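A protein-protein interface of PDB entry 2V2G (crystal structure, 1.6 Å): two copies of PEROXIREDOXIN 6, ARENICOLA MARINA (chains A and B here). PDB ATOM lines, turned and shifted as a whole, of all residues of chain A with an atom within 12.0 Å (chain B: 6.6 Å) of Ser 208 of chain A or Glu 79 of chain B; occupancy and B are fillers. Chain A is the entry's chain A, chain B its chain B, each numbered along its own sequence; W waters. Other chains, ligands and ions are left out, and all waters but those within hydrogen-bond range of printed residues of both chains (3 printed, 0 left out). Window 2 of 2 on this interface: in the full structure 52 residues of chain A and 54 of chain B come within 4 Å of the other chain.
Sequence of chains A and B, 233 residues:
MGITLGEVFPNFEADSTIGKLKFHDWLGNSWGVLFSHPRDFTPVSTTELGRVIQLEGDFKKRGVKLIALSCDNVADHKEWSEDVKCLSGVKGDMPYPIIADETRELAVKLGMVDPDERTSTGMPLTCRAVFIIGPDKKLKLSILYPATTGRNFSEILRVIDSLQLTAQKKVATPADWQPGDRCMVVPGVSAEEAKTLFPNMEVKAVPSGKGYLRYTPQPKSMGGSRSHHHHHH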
ATOM      1  N   VAL A 203      21.863 -28.685  -8.708  1.00  0.00           N
ATOM      2  CA  VAL A 203      21.461 -27.273  -8.611  1.00  0.00           C
ATOM      3  C   VAL A 203      21.928 -26.821  -7.225  1.00  0.00           C
ATOM      4  O   VAL A 203      21.412 -27.285  -6.215  1.00  0.00           O
ATOM      5  CB  VAL A 203      19.946 -27.045  -8.827  1.00  0.00           C
ATOM      6  CG1 VAL A 203      19.564 -25.546  -8.762  1.00  0.00           C
ATOM      7  CG2 VAL A 203      19.534 -27.662 -10.137  1.00  0.00           C
ATOM      8  N   LYS A 204      22.925 -25.943  -7.203  1.00  0.00           N
ATOM      9  CA  LYS A 204      23.432 -25.373  -5.942  1.00  0.00           C
ATOM     10  C   LYS A 204      22.630 -24.128  -5.476  1.00  0.00           C
ATOM     11  O   LYS A 204      22.506 -23.171  -6.207  1.00  0.00           O
ATOM     12  CB  LYS A 204      24.880 -24.989  -6.074  1.00  0.00           C
ATOM     13  CG  LYS A 204      25.470 -24.467  -4.766  1.00  0.00           C
ATOM     14  CD  LYS A 204      26.925 -24.084  -4.962  1.00  0.00           C
ATOM     15  CE  LYS A 204      27.742 -24.002  -3.650  1.00  0.00           C
ATOM     16  NZ  LYS A 204      27.334 -22.883  -2.734  1.00  0.00           N
ATOM     17  N   ALA A 205      22.108 -24.172  -4.244  1.00  0.00           N
ATOM     18  CA  ALA A 205      21.310 -23.067  -3.719  1.00  0.00           C
ATOM     19  C   ALA A 205      22.222 -21.878  -3.472  1.00  0.00           C
ATOM     20  O   ALA A 205      23.334 -22.032  -2.984  1.00  0.00           O
ATOM     21  CB  ALA A 205      20.586 -23.461  -2.446  1.00  0.00           C
ATOM     22  N   VAL A 206      21.744 -20.698  -3.856  1.00  0.00           N
ATOM     23  CA  VAL A 206      22.470 -19.421  -3.704  1.00  0.00           C
ATOM     24  C   VAL A 206      21.506 -18.408  -3.049  1.00  0.00           C
ATOM     25  O   VAL A 206      20.307 -18.618  -3.066  1.00  0.00           O
ATOM     26  CB  VAL A 206      23.034 -18.918  -5.063  1.00  0.00           C
ATOM     27  CG1 VAL A 206      24.155 -19.879  -5.533  1.00  0.00           C
ATOM     28  CG2 VAL A 206      21.916 -18.775  -6.098  1.00  0.00           C
ATOM     29  N   PRO A 207      22.026 -17.346  -2.408  1.00  0.00           N
ATOM     30  CA  PRO A 207      21.215 -16.364  -1.703  1.00  0.00           C
ATOM     31  C   PRO A 207      20.066 -15.724  -2.512  1.00  0.00           C
ATOM     32  O   PRO A 207      19.033 -15.411  -1.914  1.00  0.00           O
ATOM     33  CB  PRO A 207      22.252 -15.317  -1.275  1.00  0.00           C
ATOM     34  CG  PRO A 207      23.523 -16.049  -1.234  1.00  0.00           C
ATOM     35  CD  PRO A 207      23.467 -17.050  -2.290  1.00  0.00           C
ATOM     36  N   SER A 208      20.244 -15.568  -3.829  1.00  0.00           N
ATOM     37  CA  SER A 208      19.206 -14.958  -4.710  1.00  0.00           C
ATOM     38  C   SER A 208      17.989 -15.910  -4.810  1.00  0.00           C
ATOM     39  O   SER A 208      16.882 -15.483  -5.149  1.00  0.00           O
ATOM     40  CB  SER A 208      19.735 -14.634  -6.093  1.00  0.00           C
ATOM     41  OG  SER A 208      20.177 -15.795  -6.746  1.00  0.00           O
ATOM     42  N   GLY A 209      18.234 -17.190  -4.519  1.00  0.00           N
ATOM     43  CA  GLY A 209      17.236 -18.231  -4.575  1.00  0.00           C
ATOM     44  C   GLY A 209      16.979 -18.680  -6.003  1.00  0.00           C
ATOM     45  O   GLY A 209      16.047 -19.466  -6.235  1.00  0.00           O
ATOM     46  N   LYS A 210      17.769 -18.172  -6.940  1.00  0.00           N
ATOM     47  CA  LYS A 210      17.583 -18.449  -8.356  1.00  0.00           C
ATOM     48  C   LYS A 210      18.233 -19.827  -8.605  1.00  0.00           C
ATOM     49  O   LYS A 210      19.028 -20.338  -7.785  1.00  0.00           O
ATOM     50  CB  LYS A 210      18.163 -17.325  -9.241  1.00  0.00           C
ATOM     51  CG  LYS A 210      17.536 -15.949  -9.050  1.00  0.00           C
ATOM     52  CD  LYS A 210      18.206 -14.926  -9.904  1.00  0.00           C
ATOM     53  CE  LYS A 210      17.770 -13.528  -9.615  1.00  0.00           C
ATOM     54  NZ  LYS A 210      16.370 -13.309  -9.925  1.00  0.00           N
ATOM     55  N   GLY A 211      17.953 -20.420  -9.753  1.00  0.00           N
ATOM     56  CA  GLY A 211      18.336 -21.823  -9.951  1.00  0.00           C
ATOM     57  C   GLY A 211      19.340 -22.075 -11.052  1.00  0.00           C
ATOM     58  O   GLY A 211      19.345 -23.149 -11.613  1.00  0.00           O
ATOM     59  N   TYR A 212      20.249 -21.129 -11.246  1.00  0.00           N
ATOM     60  CA  TYR A 212      21.162 -21.091 -12.373  1.00  0.00           C
ATOM     61  C   TYR A 212      22.520 -21.779 -12.126  1.00  0.00           C
ATOM     62  O   TYR A 212      23.283 -22.045 -13.054  1.00  0.00           O
ATOM     63  CB  TYR A 212      21.392 -19.650 -12.799  1.00  0.00           C
ATOM     64  CG  TYR A 212      22.124 -18.823 -11.760  1.00  0.00           C
ATOM     65  CD1 TYR A 212      23.527 -18.826 -11.698  1.00  0.00           C
ATOM     66  CD2 TYR A 212      21.420 -18.058 -10.851  1.00  0.00           C
ATOM     67  CE1 TYR A 212      24.194 -18.089 -10.770  1.00  0.00           C
ATOM     68  CE2 TYR A 212      22.079 -17.313  -9.876  1.00  0.00           C
ATOM     69  CZ  TYR A 212      23.472 -17.365  -9.850  1.00  0.00           C
ATOM     70  OH  TYR A 212      24.153 -16.623  -8.943  1.00  0.00           O
ATOM     71  N   LEU A 213      22.824 -22.007 -10.848  1.00  0.00           N
ATOM     72  CA  LEU A 213      24.162 -22.505 -10.501  1.00  0.00           C
ATOM     73  C   LEU A 213      24.125 -24.054 -10.579  1.00  0.00           C
ATOM     74  O   LEU A 213      23.885 -24.775  -9.595  1.00  0.00           O
ATOM     75  CB  LEU A 213      24.587 -22.052  -9.104  1.00  0.00           C
ATOM     76  CG  LEU A 213      26.096 -22.017  -8.866  1.00  0.00           C
ATOM     77  CD1 LEU A 213      26.858 -21.119  -9.767  1.00  0.00           C
ATOM     78  CD2 LEU A 213      26.314 -21.524  -7.446  1.00  0.00           C
ATOM     79  N   ARG A 214      24.304 -24.547 -11.808  1.00  0.00           N
ATOM     80  CA  ARG A 214      24.045 -25.930 -12.150  1.00  0.00           C
ATOM     81  C   ARG A 214      25.292 -26.615 -12.688  1.00  0.00           C
ATOM     82  O   ARG A 214      25.824 -26.230 -13.719  1.00  0.00           O
ATOM     83  CB  ARG A 214      22.869 -26.032 -13.170  1.00  0.00           C
ATOM     84  CG  ARG A 214      21.555 -25.468 -12.580  1.00  0.00           C
ATOM     85  CD  ARG A 214      20.349 -25.720 -13.518  1.00  0.00           C
ATOM     86  NE  ARG A 214      20.528 -25.074 -14.779  1.00  0.00           N
ATOM     87  CZ  ARG A 214      19.732 -25.218 -15.835  1.00  0.00           C
ATOM     88  NH1 ARG A 214      18.688 -26.023 -15.779  1.00  0.00           N
ATOM     89  NH2 ARG A 214      20.001 -24.578 -16.951  1.00  0.00           N
ATOM     90  N   PHE B  41      23.854 -13.486 -12.811  1.00  0.00           N
ATOM     91  CA  PHE B  41      23.029 -14.653 -12.530  1.00  0.00           C
ATOM     92  C   PHE B  41      23.228 -15.769 -13.565  1.00  0.00           C
ATOM     93  O   PHE B  41      22.260 -16.475 -13.971  1.00  0.00           O
ATOM     94  CB  PHE B  41      21.549 -14.283 -12.427  1.00  0.00           C
ATOM     95  CG  PHE B  41      21.259 -13.210 -11.453  1.00  0.00           C
ATOM     96  CD1 PHE B  41      21.372 -13.451 -10.093  1.00  0.00           C
ATOM     97  CD2 PHE B  41      20.785 -11.979 -11.887  1.00  0.00           C
ATOM     98  CE1 PHE B  41      21.055 -12.454  -9.152  1.00  0.00           C
ATOM     99  CE2 PHE B  41      20.498 -10.952 -10.940  1.00  0.00           C
ATOM    100  CZ  PHE B  41      20.595 -11.217  -9.584  1.00  0.00           C
ATOM    101  N   VAL B  74      22.802  -1.875 -12.277  1.00  0.00           N
ATOM    102  CA  VAL B  74      23.550  -1.895 -10.994  1.00  0.00           C
ATOM    103  C   VAL B  74      22.746  -2.657  -9.908  1.00  0.00           C
ATOM    104  O   VAL B  74      23.365  -3.373  -9.108  1.00  0.00           O
ATOM    105  CB  VAL B  74      23.886  -0.470 -10.598  1.00  0.00           C
ATOM    106  CG1 VAL B  74      24.271  -0.325  -9.083  1.00  0.00           C
ATOM    107  CG2 VAL B  74      24.948   0.087 -11.480  1.00  0.00           C
ATOM    108  N   ALA B  75      21.423  -2.547  -9.911  1.00  0.00           N
ATOM    109  CA  ALA B  75      20.571  -3.295  -8.967  1.00  0.00           C
ATOM    110  C   ALA B  75      20.853  -4.814  -9.067  1.00  0.00           C
ATOM    111  O   ALA B  75      21.062  -5.505  -8.040  1.00  0.00           O
ATOM    112  CB  ALA B  75      19.124  -2.998  -9.202  1.00  0.00           C
ATOM    113  N   ASP B  76      20.867  -5.344 -10.299  1.00  0.00           N
ATOM    114  CA  ASP B  76      21.226  -6.740 -10.572  1.00  0.00           C
ATOM    115  C   ASP B  76      22.625  -7.058 -10.111  1.00  0.00           C
ATOM    116  O   ASP B  76      22.868  -8.092  -9.490  1.00  0.00           O
ATOM    117  CB  ASP B  76      21.035  -7.070 -12.059  1.00  0.00           C
ATOM    118  CG  ASP B  76      19.549  -7.298 -12.418  1.00  0.00           C
ATOM    119  OD1 ASP B  76      18.670  -7.283 -11.496  1.00  0.00           O
ATOM    120  OD2 ASP B  76      19.250  -7.499 -13.624  1.00  0.00           O
ATOM    121  N   HIS B  77      23.573  -6.174 -10.396  1.00  0.00           N
ATOM    122  CA  HIS B  77      24.975  -6.347  -9.942  1.00  0.00           C
ATOM    123  C   HIS B  77      25.024  -6.526  -8.435  1.00  0.00           C
ATOM    124  O   HIS B  77      25.676  -7.464  -7.932  1.00  0.00           O
ATOM    125  CB  HIS B  77      25.881  -5.165 -10.329  1.00  0.00           C
ATOM    126  CG  HIS B  77      26.141  -5.100 -11.790  1.00  0.00           C
ATOM    127  ND1 HIS B  77      26.747  -4.045 -12.431  1.00  0.00           N
ATOM    128  CD2 HIS B  77      25.915  -6.051 -12.727  1.00  0.00           C
ATOM    129  CE1 HIS B  77      26.880  -4.364 -13.723  1.00  0.00           C
ATOM    130  NE2 HIS B  77      26.413  -5.582 -13.911  1.00  0.00           N
ATOM    131  N   LYS B  78      24.308  -5.660  -7.725  1.00  0.00           N
ATOM    132  CA  LYS B  78      24.333  -5.720  -6.287  1.00  0.00           C
ATOM    133  C   LYS B  78      23.720  -7.005  -5.735  1.00  0.00           C
ATOM    134  O   LYS B  78      24.333  -7.661  -4.884  1.00  0.00           O
ATOM    135  CB  LYS B  78      23.703  -4.464  -5.673  1.00  0.00           C
ATOM    136  CG  LYS B  78      24.535  -3.276  -5.854  1.00  0.00           C
ATOM    137  CD  LYS B  78      23.975  -2.093  -5.170  1.00  0.00           C
ATOM    138  CE  LYS B  78      24.882  -0.866  -5.352  1.00  0.00           C
ATOM    139  NZ  LYS B  78      24.038   0.271  -4.971  1.00  0.00           N
ATOM    140  N   GLU B  79      22.582  -7.416  -6.276  1.00  0.00           N
ATOM    141  CA  GLU B  79      21.894  -8.618  -5.845  1.00  0.00           C
ATOM    142  C   GLU B  79      22.743  -9.872  -6.160  1.00  0.00           C
ATOM    143  O   GLU B  79      23.005 -10.737  -5.313  1.00  0.00           O
ATOM    144  CB  GLU B  79      20.535  -8.718  -6.534  1.00  0.00           C
ATOM    145  CG  GLU B  79      19.756  -9.873  -5.974  1.00  0.00           C
ATOM    146  CD  GLU B  79      18.441 -10.201  -6.663  1.00  0.00           C
ATOM    147  OE1 GLU B  79      18.141  -9.561  -7.712  1.00  0.00           O
ATOM    148  OE2 GLU B  79      17.775 -11.158  -6.163  1.00  0.00           O
ATOM    149  N   TRP B  80      23.199  -9.946  -7.407  1.00  0.00           N
ATOM    150  CA  TRP B  80      23.998 -11.098  -7.822  1.00  0.00           C
ATOM    151  C   TRP B  80      25.332 -11.185  -7.041  1.00  0.00           C
ATOM    152  O   TRP B  80      25.877 -12.277  -6.836  1.00  0.00           O
ATOM    153  CB  TRP B  80      24.270 -10.975  -9.289  1.00  0.00           C
ATOM    154  CG  TRP B  80      25.133 -12.102  -9.849  1.00  0.00           C
ATOM    155  CD1 TRP B  80      24.940 -13.441  -9.699  1.00  0.00           C
ATOM    156  CD2 TRP B  80      26.273 -11.931 -10.640  1.00  0.00           C
ATOM    157  NE1 TRP B  80      25.920 -14.144 -10.392  1.00  0.00           N
ATOM    158  CE2 TRP B  80      26.771 -13.239 -10.963  1.00  0.00           C
ATOM    159  CE3 TRP B  80      26.987 -10.817 -11.075  1.00  0.00           C
ATOM    160  CZ2 TRP B  80      27.904 -13.418 -11.762  1.00  0.00           C
ATOM    161  CZ3 TRP B  80      28.116 -11.021 -11.880  1.00  0.00           C
ATOM    162  CH2 TRP B  80      28.575 -12.296 -12.168  1.00  0.00           C
ATOM    163  N   SER B  81      25.865 -10.043  -6.647  1.00  0.00           N
ATOM    164  CA  SER B  81      27.136  -9.986  -5.882  1.00  0.00           C
ATOM    165  C   SER B  81      27.092 -10.828  -4.606  1.00  0.00           C
ATOM    166  O   SER B  81      28.098 -11.403  -4.179  1.00  0.00           O
ATOM    167  CB  SER B  81      27.520  -8.541  -5.571  1.00  0.00           C
ATOM    168  OG  SER B  81      28.075  -7.925  -6.718  1.00  0.00           O
ATOM    169  N   GLU B  82      25.904 -10.931  -4.007  1.00  0.00           N
ATOM    170  CA  GLU B  82      25.721 -11.786  -2.840  1.00  0.00           C
ATOM    171  C   GLU B  82      25.891 -13.265  -3.187  1.00  0.00           C
ATOM    172  O   GLU B  82      26.473 -14.003  -2.385  1.00  0.00           O
ATOM    173  CB  GLU B  82      24.402 -11.448  -2.177  1.00  0.00           C
ATOM    174  CG  GLU B  82      24.351 -10.003  -1.691  1.00  0.00           C
ATOM    175  CD  GLU B  82      25.470  -9.684  -0.691  1.00  0.00           C
ATOM    176  OE1 GLU B  82      25.578 -10.396   0.327  1.00  0.00           O
ATOM    177  OE2 GLU B  82      26.252  -8.747  -0.937  1.00  0.00           O
ATOM    178  N   ASP B  83      25.447 -13.694  -4.368  1.00  0.00           N
ATOM    179  CA  ASP B  83      25.726 -15.053  -4.866  1.00  0.00           C
ATOM    180  C   ASP B  83      27.220 -15.287  -5.129  1.00  0.00           C
ATOM    181  O   ASP B  83      27.775 -16.392  -4.839  1.00  0.00           O
ATOM    182  CB  ASP B  83      24.933 -15.343  -6.166  1.00  0.00           C
ATOM    183  CG  ASP B  83      23.397 -15.341  -5.969  1.00  0.00           C
ATOM    184  OD1 ASP B  83      22.924 -15.173  -4.833  1.00  0.00           O
ATOM    185  OD2 ASP B  83      22.706 -15.445  -7.031  1.00  0.00           O
ATOM    186  N   VAL B  84      27.870 -14.274  -5.677  1.00  0.00           N
ATOM    187  CA  VAL B  84      29.304 -14.332  -6.004  1.00  0.00           C
ATOM    188  C   VAL B  84      30.067 -14.455  -4.716  1.00  0.00           C
ATOM    189  O   VAL B  84      31.005 -15.250  -4.663  1.00  0.00           O
ATOM    190  CB  VAL B  84      29.787 -13.121  -6.755  1.00  0.00           C
ATOM    191  CG1 VAL B  84      31.320 -13.052  -6.895  1.00  0.00           C
ATOM    192  CG2 VAL B  84      29.098 -13.137  -8.163  1.00  0.00           C
HETATM  193  O   HOH W   1      16.251 -13.058  -6.590  1.00  0.00           O
HETATM  194  O   HOH W   2      21.692 -12.654  -3.994  1.00  0.00           O
HETATM  195  O   HOH W   3      16.173 -10.464  -9.347  1.00  0.00           O
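Of the printed residues of chain B, Ser 208 of chain A touches Phe 41, Glu 79 and Asp 83.
Printed residues of chain B within 4 Å of Tyr 212 of chain A: Phe 41, Trp 80 and Asp 83.
Printed residues of chain A within 4 Å of Phe 41 of chain B: Ser 208 (3.98 Å), Lys 210 (3.5 Å) and Tyr 212 (3.2 Å).
Ala 75 of chain B touches none of the printed residues of chain A.
No residue of chain A comes within 4 Å of Asp 76 of chain B.
No residue of chain A comes within 4 Å of Lys 78 of chain B.
Printed residues of chain A within 4 Å of Glu 79 of chain B: Ser 208.
Of chain A, only Pro 207 (3.8 Å) comes within 4 Å of Glu 82 of chain B.
Of chain A, only Val 206, Pro 207, Ser 208 and Tyr 212 come within 4 Å of Asp 83 of chain B.
The nearest printed residue of chain B that does not touch Ser 208 of chain A is Trp 80 of chain B (5.8 Å).
The nearest printed residue of chain A that does not touch Glu 79 of chain B is Lys 210 of chain A (4.2 Å).
Water W1 lies within hydrogen-bond range of the side-chain carboxylate (OE2) of Glu 79 of chain B (2.5 Å), the backbone carbonyl oxygen (O) of Ser 208 of chain A (2.9 Å) and the side-chain amino group (NZ) of Lys 210 of chain A (3.3 Å).
Water W2 lies within hydrogen-bond range of O of Glu 79 of chain B, OD1 of Asp 83 of chain B and N of Ser 208 of chain A.
Water W3 bridges OE1 of Glu 79 of chain B (2.7 Å) and NZ of Lys 210 of chain A (2.9 Å).
No position is printed for both chains.
Of the 10 pairs that touch across the chains among the printed residues, none has its exchanged pair printed and touching as well.
The side-chain hydroxyl (OG) of Ser 208 of chain A lies close to the backbone NH (N) of Lys 210 of chain A.
Asp 83 of chain B touches Val 206 of chain A.
Pro 207 of chain A touches Glu 82 of chain B (CG to O, 3.8 Å).
CB of Ser 208 of chain A touches CE1 of Phe 41 of chain B (3.98 Å).
CB of Ser 208 of chain A touches OE2 of Glu 79 of chain B, at 3.99 Å.
Phe 41 of chain B touches Lys 210 of chain A (CE1 to CE, 3.5 Å).
Phe 41 of chain B touches Tyr 212 of chain A (O to CG, 3.2 Å).
Printed residues of chain A that touch a printed residue of chain B: Val 206, Pro 207, Ser 208, Lys 210 and Tyr 212.
Hydrophobic or aromatic side chains of chain A that line the printed part of chain B: Val 206, Pro 207 and Tyr 212.
Hydrophobic or aromatic side chains of chain B within 4 Å of the printed part of chain A: Phe 41 and Trp 80.
Among the printed residues, 10 pairs touch across the chains.
OG of Ser 208 of chain A is in hydrogen-bond range of OD2 of Asp 83 of chain B (2.6 Å).
The side-chain hydroxyl of Tyr 212 of chain A sits close to the indole nitrogen of Trp 80 of chain B.
The side-chain hydroxyl (OH) of Tyr 212 of chain A lies within hydrogen-bond range of the side-chain carboxylate (OD2) of Asp 83 of chain B, at 2.7 Å.
N of Pro 207 of chain A sits close to OD1 of Asp 83 of chain B, 3.4 Å away.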
